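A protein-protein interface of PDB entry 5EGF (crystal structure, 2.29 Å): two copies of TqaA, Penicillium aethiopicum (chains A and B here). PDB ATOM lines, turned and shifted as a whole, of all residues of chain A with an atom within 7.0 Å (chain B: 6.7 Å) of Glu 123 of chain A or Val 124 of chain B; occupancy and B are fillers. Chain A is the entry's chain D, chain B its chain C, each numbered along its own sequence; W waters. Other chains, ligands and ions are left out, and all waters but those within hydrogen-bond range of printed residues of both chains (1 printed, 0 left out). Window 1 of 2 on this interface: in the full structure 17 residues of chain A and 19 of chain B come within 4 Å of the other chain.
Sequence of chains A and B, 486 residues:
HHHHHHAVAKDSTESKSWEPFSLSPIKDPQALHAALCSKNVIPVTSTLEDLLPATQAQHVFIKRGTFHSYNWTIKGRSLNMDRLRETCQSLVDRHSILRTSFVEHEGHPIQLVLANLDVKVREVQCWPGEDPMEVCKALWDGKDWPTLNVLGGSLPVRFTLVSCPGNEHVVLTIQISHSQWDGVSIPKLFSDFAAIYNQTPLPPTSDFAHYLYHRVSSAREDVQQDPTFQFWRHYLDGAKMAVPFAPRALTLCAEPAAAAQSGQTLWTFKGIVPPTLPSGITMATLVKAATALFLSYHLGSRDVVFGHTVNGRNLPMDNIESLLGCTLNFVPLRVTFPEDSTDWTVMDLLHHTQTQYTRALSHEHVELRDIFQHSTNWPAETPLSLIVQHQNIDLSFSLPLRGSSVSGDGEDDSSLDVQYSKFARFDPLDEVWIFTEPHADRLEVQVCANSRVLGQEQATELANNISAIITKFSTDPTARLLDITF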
ATOM      1  N   MET A  81      27.978   2.158  -1.494  1.00  0.00           N
ATOM      2  CA  MET A  81      27.095   3.304  -1.290  1.00  0.00           C
ATOM      3  C   MET A  81      25.792   3.152  -2.042  1.00  0.00           C
ATOM      4  O   MET A  81      24.726   3.448  -1.505  1.00  0.00           O
ATOM      5  CB  MET A  81      27.783   4.600  -1.723  1.00  0.00           C
ATOM      6  CG  MET A  81      29.024   4.920  -0.922  1.00  0.00           C
ATOM      7  SD  MET A  81      28.607   5.538   0.874  1.00  0.00           S
ATOM      8  CE  MET A  81      28.039   7.339   0.353  1.00  0.00           C
ATOM      9  N   ASP A  82      25.872   2.711  -3.293  1.00  0.00           N
ATOM     10  CA  ASP A  82      24.655   2.478  -4.065  1.00  0.00           C
ATOM     11  C   ASP A  82      23.791   1.384  -3.449  1.00  0.00           C
ATOM     12  O   ASP A  82      22.589   1.366  -3.647  1.00  0.00           O
ATOM     13  CB  ASP A  82      24.962   2.160  -5.526  1.00  0.00           C
ATOM     14  CG  ASP A  82      25.239   3.405  -6.347  1.00  0.00           C
ATOM     15  OD1 ASP A  82      25.047   4.517  -5.821  1.00  0.00           O
ATOM     16  OD2 ASP A  82      25.641   3.270  -7.525  1.00  0.00           O
ATOM     17  N   ARG A  85      21.975   2.965  -0.430  1.00  0.00           N
ATOM     18  CA  ARG A  85      20.852   3.734  -0.947  1.00  0.00           C
ATOM     19  C   ARG A  85      19.720   2.806  -1.344  1.00  0.00           C
ATOM     20  O   ARG A  85      18.563   3.056  -1.003  1.00  0.00           O
ATOM     21  CB  ARG A  85      21.265   4.577  -2.149  1.00  0.00           C
ATOM     22  CG  ARG A  85      22.447   5.490  -1.914  1.00  0.00           C
ATOM     23  CD  ARG A  85      22.842   6.164  -3.221  1.00  0.00           C
ATOM     24  NE  ARG A  85      23.893   7.160  -3.036  1.00  0.00           N
ATOM     25  CZ  ARG A  85      25.188   6.938  -3.252  1.00  0.00           C
ATOM     26  NH1 ARG A  85      25.604   5.749  -3.666  1.00  0.00           N
ATOM     27  NH2 ARG A  85      26.074   7.906  -3.056  1.00  0.00           N
ATOM     28  N   VAL A 121      17.351   9.844  -0.596  1.00  0.00           N
ATOM     29  CA  VAL A 121      18.285  10.042   0.512  1.00  0.00           C
ATOM     30  C   VAL A 121      18.766  11.492   0.506  1.00  0.00           C
ATOM     31  O   VAL A 121      18.910  12.097  -0.560  1.00  0.00           O
ATOM     32  CB  VAL A 121      19.521   9.140   0.362  1.00  0.00           C
ATOM     33  CG1 VAL A 121      20.221   8.917   1.711  1.00  0.00           C
ATOM     34  CG2 VAL A 121      19.135   7.819  -0.283  1.00  0.00           C
ATOM     35  N   ARG A 122      19.000  12.057   1.686  1.00  0.00           N
ATOM     36  CA  ARG A 122      19.696  13.337   1.759  1.00  0.00           C
ATOM     37  C   ARG A 122      21.184  13.005   1.895  1.00  0.00           C
ATOM     38  O   ARG A 122      21.577  12.208   2.762  1.00  0.00           O
ATOM     39  CB  ARG A 122      19.193  14.187   2.923  1.00  0.00           C
ATOM     40  CG  ARG A 122      20.029  15.427   3.204  1.00  0.00           C
ATOM     41  CD  ARG A 122      19.400  16.267   4.311  1.00  0.00           C
ATOM     42  NE  ARG A 122      19.462  15.633   5.634  1.00  0.00           N
ATOM     43  CZ  ARG A 122      18.926  16.151   6.738  1.00  0.00           C
ATOM     44  NH1 ARG A 122      18.281  17.306   6.678  1.00  0.00           N
ATOM     45  NH2 ARG A 122      19.035  15.514   7.898  1.00  0.00           N
ATOM     46  N   GLU A 123      21.997  13.563   1.002  1.00  0.00           N
ATOM     47  CA  GLU A 123      23.418  13.228   0.979  1.00  0.00           C
ATOM     48  C   GLU A 123      24.367  14.412   1.225  1.00  0.00           C
ATOM     49  O   GLU A 123      24.199  15.505   0.669  1.00  0.00           O
ATOM     50  CB  GLU A 123      23.790  12.529  -0.331  1.00  0.00           C
ATOM     51  CG  GLU A 123      23.409  11.048  -0.392  1.00  0.00           C
ATOM     52  CD  GLU A 123      24.386  10.243  -1.245  1.00  0.00           C
ATOM     53  OE1 GLU A 123      25.334   9.627  -0.689  1.00  0.00           O
ATOM     54  OE2 GLU A 123      24.212  10.244  -2.480  1.00  0.00           O
ATOM     55  N   VAL A 124      25.379  14.168   2.053  1.00  0.00           N
ATOM     56  CA  VAL A 124      26.401  15.168   2.318  1.00  0.00           C
ATOM     57  C   VAL A 124      27.778  14.616   2.031  1.00  0.00           C
ATOM     58  O   VAL A 124      28.179  13.597   2.611  1.00  0.00           O
ATOM     59  CB  VAL A 124      26.394  15.660   3.785  1.00  0.00           C
ATOM     60  CG1 VAL A 124      27.386  16.833   3.970  1.00  0.00           C
ATOM     61  CG2 VAL A 124      24.996  16.075   4.206  1.00  0.00           C
ATOM     62  N   GLN A 125      28.494  15.299   1.138  1.00  0.00           N
ATOM     63  CA  GLN A 125      29.923  15.076   0.920  1.00  0.00           C
ATOM     64  C   GLN A 125      30.677  16.108   1.765  1.00  0.00           C
ATOM     65  O   GLN A 125      30.690  17.304   1.433  1.00  0.00           O
ATOM     66  CB  GLN A 125      30.273  15.225  -0.572  1.00  0.00           C
ATOM     67  CG  GLN A 125      29.781  14.071  -1.502  1.00  0.00           C
ATOM     68  CD  GLN A 125      28.302  14.162  -1.942  1.00  0.00           C
ATOM     69  OE1 GLN A 125      27.902  15.092  -2.647  1.00  0.00           O
ATOM     70  NE2 GLN A 125      27.499  13.163  -1.548  1.00  0.00           N
ATOM     71  N   VAL A 135      28.173  17.143  11.500  1.00  0.00           N
ATOM     72  CA  VAL A 135      27.258  17.624  10.465  1.00  0.00           C
ATOM     73  C   VAL A 135      25.814  17.152  10.697  1.00  0.00           C
ATOM     74  O   VAL A 135      24.862  17.928  10.560  1.00  0.00           O
ATOM     75  CB  VAL A 135      27.722  17.231   9.057  1.00  0.00           C
ATOM     76  CG1 VAL A 135      26.555  17.346   8.084  1.00  0.00           C
ATOM     77  CG2 VAL A 135      28.892  18.115   8.617  1.00  0.00           C
ATOM     78  N   LEU A 139      22.331  19.501  11.434  1.00  0.00           N
ATOM     79  CA  LEU A 139      21.114  19.529  10.630  1.00  0.00           C
ATOM     80  C   LEU A 139      19.948  19.222  11.557  1.00  0.00           C
ATOM     81  O   LEU A 139      18.885  19.812  11.433  1.00  0.00           O
ATOM     82  CB  LEU A 139      21.207  18.564   9.441  1.00  0.00           C
ATOM     83  CG  LEU A 139      22.300  18.915   8.428  1.00  0.00           C
ATOM     84  CD1 LEU A 139      22.541  17.768   7.467  1.00  0.00           C
ATOM     85  CD2 LEU A 139      21.930  20.179   7.678  1.00  0.00           C
ATOM     86  N   PHE A 159      15.933   9.204   5.244  1.00  0.00           N
ATOM     87  CA  PHE A 159      17.300   8.737   5.425  1.00  0.00           C
ATOM     88  C   PHE A 159      18.295   9.816   5.075  1.00  0.00           C
ATOM     89  O   PHE A 159      18.067  10.604   4.149  1.00  0.00           O
ATOM     90  CB  PHE A 159      17.556   7.516   4.544  1.00  0.00           C
ATOM     91  CG  PHE A 159      16.682   6.351   4.870  1.00  0.00           C
ATOM     92  CD1 PHE A 159      15.380   6.287   4.385  1.00  0.00           C
ATOM     93  CD2 PHE A 159      17.147   5.319   5.670  1.00  0.00           C
ATOM     94  CE1 PHE A 159      14.563   5.205   4.691  1.00  0.00           C
ATOM     95  CE2 PHE A 159      16.334   4.237   5.971  1.00  0.00           C
ATOM     96  CZ  PHE A 159      15.043   4.184   5.485  1.00  0.00           C
ATOM     97  N   THR A 160      19.404   9.840   5.808  1.00  0.00           N
ATOM     98  CA  THR A 160      20.510  10.744   5.498  1.00  0.00           C
ATOM     99  C   THR A 160      21.855  10.013   5.469  1.00  0.00           C
ATOM    100  O   THR A 160      22.144   9.172   6.341  1.00  0.00           O
ATOM    101  CB  THR A 160      20.559  11.944   6.479  1.00  0.00           C
ATOM    102  OG1 THR A 160      19.416  12.772   6.252  1.00  0.00           O
ATOM    103  CG2 THR A 160      21.816  12.803   6.250  1.00  0.00           C
ATOM    104  N   LEU A 161      22.663  10.343   4.457  1.00  0.00           N
ATOM    105  CA  LEU A 161      23.988   9.752   4.275  1.00  0.00           C
ATOM    106  C   LEU A 161      25.082  10.824   4.258  1.00  0.00           C
ATOM    107  O   LEU A 161      25.163  11.622   3.313  1.00  0.00           O
ATOM    108  CB  LEU A 161      24.030   8.965   2.967  1.00  0.00           C
ATOM    109  CG  LEU A 161      24.991   7.779   2.970  1.00  0.00           C
ATOM    110  CD1 LEU A 161      24.683   6.911   4.172  1.00  0.00           C
ATOM    111  CD2 LEU A 161      24.876   6.972   1.681  1.00  0.00           C
ATOM    112  N   VAL A 162      25.920  10.838   5.296  1.00  0.00           N
ATOM    113  CA  VAL A 162      27.007  11.837   5.426  1.00  0.00           C
ATOM    114  C   VAL A 162      28.409  11.200   5.338  1.00  0.00           C
ATOM    115  O   VAL A 162      28.778  10.396   6.197  1.00  0.00           O
ATOM    116  CB  VAL A 162      26.922  12.607   6.770  1.00  0.00           C
ATOM    117  CG1 VAL A 162      27.845  13.826   6.752  1.00  0.00           C
ATOM    118  CG2 VAL A 162      25.487  13.042   7.077  1.00  0.00           C
ATOM    119  N   SER A 163      29.191  11.588   4.329  1.00  0.00           N
ATOM    120  CA  SER A 163      30.439  10.884   3.993  1.00  0.00           C
ATOM    121  C   SER A 163      31.729  11.703   4.114  1.00  0.00           C
ATOM    122  O   SER A 163      31.824  12.793   3.549  1.00  0.00           O
ATOM    123  CB  SER A 163      30.369  10.363   2.546  1.00  0.00           C
ATOM    124  OG  SER A 163      29.421   9.325   2.411  1.00  0.00           O
ATOM    125  N   ASN A 167      34.599   7.875   1.508  1.00  0.00           N
ATOM    126  CA  ASN A 167      33.494   6.952   1.796  1.00  0.00           C
ATOM    127  C   ASN A 167      33.885   5.770   2.688  1.00  0.00           C
ATOM    128  O   ASN A 167      33.239   4.720   2.667  1.00  0.00           O
ATOM    129  CB  ASN A 167      32.808   6.470   0.512  1.00  0.00           C
ATOM    130  CG  ASN A 167      32.105   7.593  -0.225  1.00  0.00           C
ATOM    131  OD1 ASN A 167      31.479   8.466   0.392  1.00  0.00           O
ATOM    132  ND2 ASN A 167      32.210   7.591  -1.550  1.00  0.00           N
ATOM    133  N   MET B  81      27.189  21.633 -12.966  1.00  0.00           N
ATOM    134  CA  MET B  81      27.715  21.343 -11.642  1.00  0.00           C
ATOM    135  C   MET B  81      29.204  21.066 -11.699  1.00  0.00           C
ATOM    136  O   MET B  81      29.958  21.504 -10.828  1.00  0.00           O
ATOM    137  CB  MET B  81      26.994  20.140 -11.041  1.00  0.00           C
ATOM    138  CG  MET B  81      25.519  20.382 -10.829  1.00  0.00           C
ATOM    139  SD  MET B  81      25.249  21.618  -9.341  1.00  0.00           S
ATOM    140  CE  MET B  81      25.867  20.420  -7.914  1.00  0.00           C
ATOM    141  N   ARG B 122      32.279  21.077  -0.326  1.00  0.00           N
ATOM    142  CA  ARG B 122      31.341  20.361   0.530  1.00  0.00           C
ATOM    143  C   ARG B 122      29.986  20.392  -0.156  1.00  0.00           C
ATOM    144  O   ARG B 122      29.491  21.470  -0.507  1.00  0.00           O
ATOM    145  CB  ARG B 122      31.237  21.021   1.891  1.00  0.00           C
ATOM    146  CG  ARG B 122      29.996  20.608   2.667  1.00  0.00           C
ATOM    147  CD  ARG B 122      30.029  21.147   4.083  1.00  0.00           C
ATOM    148  NE  ARG B 122      29.612  22.548   4.155  1.00  0.00           N
ATOM    149  CZ  ARG B 122      29.513  23.247   5.285  1.00  0.00           C
ATOM    150  NH1 ARG B 122      29.811  22.682   6.447  1.00  0.00           N
ATOM    151  NH2 ARG B 122      29.111  24.512   5.254  1.00  0.00           N
ATOM    152  N   GLU B 123      29.395  19.217  -0.370  1.00  0.00           N
ATOM    153  CA  GLU B 123      28.205  19.139  -1.206  1.00  0.00           C
ATOM    154  C   GLU B 123      27.040  18.476  -0.513  1.00  0.00           C
ATOM    155  O   GLU B 123      27.195  17.440   0.139  1.00  0.00           O
ATOM    156  CB  GLU B 123      28.494  18.399  -2.512  1.00  0.00           C
ATOM    157  CG  GLU B 123      29.617  19.005  -3.327  1.00  0.00           C
ATOM    158  CD  GLU B 123      30.004  18.135  -4.500  1.00  0.00           C
ATOM    159  OE1 GLU B 123      29.144  17.994  -5.393  1.00  0.00           O
ATOM    160  OE2 GLU B 123      31.148  17.599  -4.533  1.00  0.00           O
ATOM    161  N   VAL B 124      25.868  19.080  -0.685  1.00  0.00           N
ATOM    162  CA  VAL B 124      24.621  18.537  -0.158  1.00  0.00           C
ATOM    163  C   VAL B 124      23.599  18.316  -1.270  1.00  0.00           C
ATOM    164  O   VAL B 124      23.280  19.256  -2.027  1.00  0.00           O
ATOM    165  CB  VAL B 124      23.962  19.483   0.885  1.00  0.00           C
ATOM    166  CG1 VAL B 124      22.665  18.861   1.426  1.00  0.00           C
ATOM    167  CG2 VAL B 124      24.929  19.825   2.019  1.00  0.00           C
ATOM    168  N   GLN B 125      23.084  17.086  -1.348  1.00  0.00           N
ATOM    169  CA  GLN B 125      21.901  16.780  -2.152  1.00  0.00           C
ATOM    170  C   GLN B 125      20.684  16.722  -1.231  1.00  0.00           C
ATOM    171  O   GLN B 125      20.536  15.787  -0.438  1.00  0.00           O
ATOM    172  CB  GLN B 125      22.068  15.456  -2.905  1.00  0.00           C
ATOM    173  CG  GLN B 125      23.164  15.457  -4.005  1.00  0.00           C
ATOM    174  CD  GLN B 125      24.600  15.421  -3.461  1.00  0.00           C
ATOM    175  OE1 GLN B 125      24.888  14.746  -2.468  1.00  0.00           O
ATOM    176  NE2 GLN B 125      25.504  16.151  -4.120  1.00  0.00           N
ATOM    177  N   CYS B 126      19.819  17.726  -1.331  1.00  0.00           N
ATOM    178  CA  CYS B 126      18.688  17.853  -0.417  1.00  0.00           C
ATOM    179  C   CYS B 126      17.548  16.854  -0.656  1.00  0.00           C
ATOM    180  O   CYS B 126      17.352  16.366  -1.769  1.00  0.00           O
ATOM    181  CB  CYS B 126      18.107  19.257  -0.502  1.00  0.00           C
ATOM    182  SG  CYS B 126      19.149  20.530   0.227  1.00  0.00           S
ATOM    183  N   TRP B 127      16.783  16.570   0.392  1.00  0.00           N
ATOM    184  CA  TRP B 127      15.517  15.878   0.219  1.00  0.00           C
ATOM    185  C   TRP B 127      14.658  16.692  -0.723  1.00  0.00           C
ATOM    186  O   TRP B 127      14.854  17.911  -0.848  1.00  0.00           O
ATOM    187  CB  TRP B 127      14.768  15.778   1.548  1.00  0.00           C
ATOM    188  CG  TRP B 127      15.285  14.711   2.434  1.00  0.00           C
ATOM    189  CD1 TRP B 127      15.660  13.455   2.068  1.00  0.00           C
ATOM    190  CD2 TRP B 127      15.496  14.803   3.848  1.00  0.00           C
ATOM    191  NE1 TRP B 127      16.081  12.751   3.170  1.00  0.00           N
ATOM    192  CE2 TRP B 127      15.996  13.558   4.274  1.00  0.00           C
ATOM    193  CE3 TRP B 127      15.304  15.814   4.792  1.00  0.00           C
ATOM    194  CZ2 TRP B 127      16.318  13.296   5.609  1.00  0.00           C
ATOM    195  CZ3 TRP B 127      15.624  15.548   6.121  1.00  0.00           C
ATOM    196  CH2 TRP B 127      16.128  14.302   6.512  1.00  0.00           C
ATOM    197  N   GLU B 130      13.015  20.130   0.633  1.00  0.00           N
ATOM    198  CA  GLU B 130      13.917  20.769   1.587  1.00  0.00           C
ATOM    199  C   GLU B 130      14.579  21.999   0.960  1.00  0.00           C
ATOM    200  O   GLU B 130      15.196  21.897  -0.090  1.00  0.00           O
ATOM    201  CB  GLU B 130      14.970  19.752   2.055  1.00  0.00           C
ATOM    202  CG  GLU B 130      15.901  20.226   3.169  1.00  0.00           C
ATOM    203  CD  GLU B 130      16.833  19.132   3.664  1.00  0.00           C
ATOM    204  OE1 GLU B 130      17.418  18.405   2.822  1.00  0.00           O
ATOM    205  OE2 GLU B 130      16.984  18.992   4.898  1.00  0.00           O
ATOM    206  N   VAL B 135      19.244  24.713   4.734  1.00  0.00           N
ATOM    207  CA  VAL B 135      20.322  23.775   4.980  1.00  0.00           C
ATOM    208  C   VAL B 135      21.641  24.529   5.248  1.00  0.00           C
ATOM    209  O   VAL B 135      22.375  24.209   6.192  1.00  0.00           O
ATOM    210  CB  VAL B 135      20.515  22.811   3.806  1.00  0.00           C
ATOM    211  CG1 VAL B 135      21.739  21.971   4.039  1.00  0.00           C
ATOM    212  CG2 VAL B 135      19.276  21.900   3.627  1.00  0.00           C
ATOM    213  N   LEU B 139      23.883  24.762   8.739  1.00  0.00           N
ATOM    214  CA  LEU B 139      25.298  24.427   8.823  1.00  0.00           C
ATOM    215  C   LEU B 139      26.044  25.605   9.444  1.00  0.00           C
ATOM    216  O   LEU B 139      26.893  25.414  10.313  1.00  0.00           O
ATOM    217  CB  LEU B 139      25.862  24.084   7.440  1.00  0.00           C
ATOM    218  CG  LEU B 139      25.239  22.854   6.766  1.00  0.00           C
ATOM    219  CD1 LEU B 139      25.808  22.669   5.366  1.00  0.00           C
ATOM    220  CD2 LEU B 139      25.414  21.576   7.599  1.00  0.00           C
ATOM    221  N   THR B 160      30.754  25.720  -0.453  1.00  0.00           N
ATOM    222  CA  THR B 160      29.636  24.806  -0.265  1.00  0.00           C
ATOM    223  C   THR B 160      28.671  24.897  -1.431  1.00  0.00           C
ATOM    224  O   THR B 160      28.474  25.969  -2.020  1.00  0.00           O
ATOM    225  CB  THR B 160      28.886  25.036   1.056  1.00  0.00           C
ATOM    226  OG1 THR B 160      29.793  24.871   2.158  1.00  0.00           O
ATOM    227  CG2 THR B 160      27.754  24.016   1.194  1.00  0.00           C
ATOM    228  N   LEU B 161      28.090  23.749  -1.761  1.00  0.00           N
ATOM    229  CA  LEU B 161      27.150  23.622  -2.867  1.00  0.00           C
ATOM    230  C   LEU B 161      25.940  22.775  -2.429  1.00  0.00           C
ATOM    231  O   LEU B 161      26.063  21.569  -2.165  1.00  0.00           O
ATOM    232  CB  LEU B 161      27.859  22.961  -4.051  1.00  0.00           C
ATOM    233  CG  LEU B 161      27.245  23.169  -5.429  1.00  0.00           C
ATOM    234  CD1 LEU B 161      26.865  24.621  -5.582  1.00  0.00           C
ATOM    235  CD2 LEU B 161      28.223  22.730  -6.527  1.00  0.00           C
ATOM    236  N   VAL B 162      24.773  23.401  -2.353  1.00  0.00           N
ATOM    237  CA  VAL B 162      23.596  22.702  -1.849  1.00  0.00           C
ATOM    238  C   VAL B 162      22.530  22.667  -2.928  1.00  0.00           C
ATOM    239  O   VAL B 162      22.083  23.719  -3.394  1.00  0.00           O
ATOM    240  CB  VAL B 162      23.009  23.382  -0.605  1.00  0.00           C
ATOM    241  CG1 VAL B 162      21.889  22.507   0.001  1.00  0.00           C
ATOM    242  CG2 VAL B 162      24.095  23.644   0.422  1.00  0.00           C
ATOM    243  N   SER B 163      22.110  21.461  -3.308  1.00  0.00           N
ATOM    244  CA  SER B 163      21.238  21.320  -4.463  1.00  0.00           C
ATOM    245  C   SER B 163      19.909  20.629  -4.191  1.00  0.00           C
ATOM    246  O   SER B 163      19.846  19.658  -3.433  1.00  0.00           O
ATOM    247  CB  SER B 163      21.981  20.556  -5.564  1.00  0.00           C
ATOM    248  OG  SER B 163      23.232  20.100  -5.094  1.00  0.00           O
ATOM    249  N   CYS B 164      18.858  21.135  -4.833  1.00  0.00           N
ATOM    250  CA  CYS B 164      17.635  20.357  -5.051  1.00  0.00           C
ATOM    251  C   CYS B 164      17.949  19.264  -6.099  1.00  0.00           C
ATOM    252  O   CYS B 164      18.785  19.473  -6.978  1.00  0.00           O
ATOM    253  CB  CYS B 164      16.487  21.263  -5.510  1.00  0.00           C
ATOM    254  SG  CYS B 164      16.076  22.626  -4.355  1.00  0.00           S
ATOM    255  N   VAL B 170      20.156  25.666  -6.911  1.00  0.00           N
ATOM    256  CA  VAL B 170      21.289  25.370  -6.053  1.00  0.00           C
ATOM    257  C   VAL B 170      21.690  26.590  -5.237  1.00  0.00           C
ATOM    258  O   VAL B 170      21.350  27.720  -5.586  1.00  0.00           O
ATOM    259  CB  VAL B 170      22.481  24.888  -6.887  1.00  0.00           C
ATOM    260  CG1 VAL B 170      23.542  24.272  -5.999  1.00  0.00           C
ATOM    261  CG2 VAL B 170      22.016  23.879  -7.919  1.00  0.00           C
HETATM  262  O   HOH W   1      17.103  13.066  -2.325  1.00  0.00           O
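Of the printed residues of chain B, Arg 122 of chain A touches Gln 125 (3.4 Å), Trp 127 (3.2 Å) and Glu 130 (2.8 Å). Leu 161 of chain A touches none of the printed residues of chain B. Of the printed residues of chain A, Val 124 of chain B touches Glu 123. Of the printed residues of chain A, Leu 139 of chain B touches Leu 139. The nearest residue of chain A that does not touch Val 124 of chain B is Val 124 of chain A (4.3 Å).
Among the printed residues, merely in contact across the chains: Glu 123 of chain A with Val 124 of chain B (3.2 Å), Thr 160 of chain A with Trp 127 of chain B (3.2 Å), Val 124 of chain A with Glu 123 of chain B (3.2 Å), Gln 125 of chain A with Arg 122 of chain B (3.3 Å), Arg 122 of chain A with Gln 125 of chain B (3.4 Å), Glu 123 of chain A with Glu 123 of chain B (3.6 Å), Leu 139 of chain A with Leu 139 of chain B (3.8 Å) and Val 121 of chain A with Trp 127 of chain B (3.99 Å).
Arg 122 of chain A touches Gln 125 of chain B, and with the chains exchanged Gln 125 of chain A touches Arg 122 of chain B. Glu 123 of chain A touches Val 124 of chain B, and with the chains exchanged Val 124 of chain A touches Glu 123 of chain B. Glu 123 of chain A touches Gln 125 of chain B, and with the chains exchanged Gln 125 of chain A touches Glu 123 of chain B. Leu 139 of chain B touches its own counterpart, Leu 139 of chain A. Of the 14 pairs that touch across the chains among the printed residues, 9 have their exchanged pair printed and touching as well.
Water W1 bridges the backbone carbonyl oxygen (O) of Val 121 of chain A (2.7 Å) and the backbone carbonyl oxygen (O) of Cys 126 of chain B (3.4 Å).
The backbone carbonyl oxygen (O) of Glu 123 of chain B is in hydrogen-bond range of the backbone NH (N) of Gln 125 of chain A (2.7 Å). The indole nitrogen of Trp 127 of chain B lies within hydrogen-bond range of the backbone carbonyl oxygen of Phe 159 of chain A (3.1 Å). NE2 of Gln 125 of chain B lies within hydrogen-bond range of OE1 of Gln 125 of chain A (3.0 Å). The backbone NH (N) of Gln 125 of chain B is in hydrogen-bond range of the backbone carbonyl oxygen (O) of Glu 123 of chain A, 2.8 Å away. NE1 of Trp 127 of chain B lies close to N of Arg 122 of chain A (3.3 Å). The side-chain carboxylate (OE2) of Glu 130 of chain B is in salt-bridge range of the guanidinium group (NH1) of Arg 122 of chain A (2.8 Å).
Of the 16 printed residues of chain A, 8 touch a printed residue of chain B. Hydrophobic or aromatic side chains of chain A that line the printed part of chain B: Val 124 and Leu 139. Of the 16 printed residues of chain B, 7 touch a printed residue of chain A. Hydrophobic or aromatic side chains of chain B that line the printed part of chain A: Val 124, Trp 127 and Leu 139. Among the printed residues, Asp or Glu carboxylates within 4 Å of a Lys or Arg side-chain nitrogen of the other chain: Arg 122 of chain A with Glu 130 of chain B (2.8 Å).
O of Val 124 of chain B lies within hydrogen-bond range of N of Ser 163 of chain B (2.8 Å). The backbone carbonyl oxygen (O) of Arg 122 of chain B lies within hydrogen-bond range of the backbone NH (N) of Leu 161 of chain B, at 3.0 Å. The backbone carbonyl oxygen (O) of Arg 122 of chain A lies within hydrogen-bond range of the backbone NH (N) of Leu 161 of chain A, at 2.7 Å. NE of Arg 122 of chain A lies within hydrogen-bond range of OG1 of Thr 160 of chain A. The side-chain carboxylate (OE1) of Glu 123 of chain A lies within salt-bridge range of the guanidinium group (NH2) of Arg 85 of chain A (3.0 Å). The backbone carbonyl oxygen (O) of Phe 159 of chain A is in hydrogen-bond range of the backbone NH (N) of Arg 122 of chain A.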
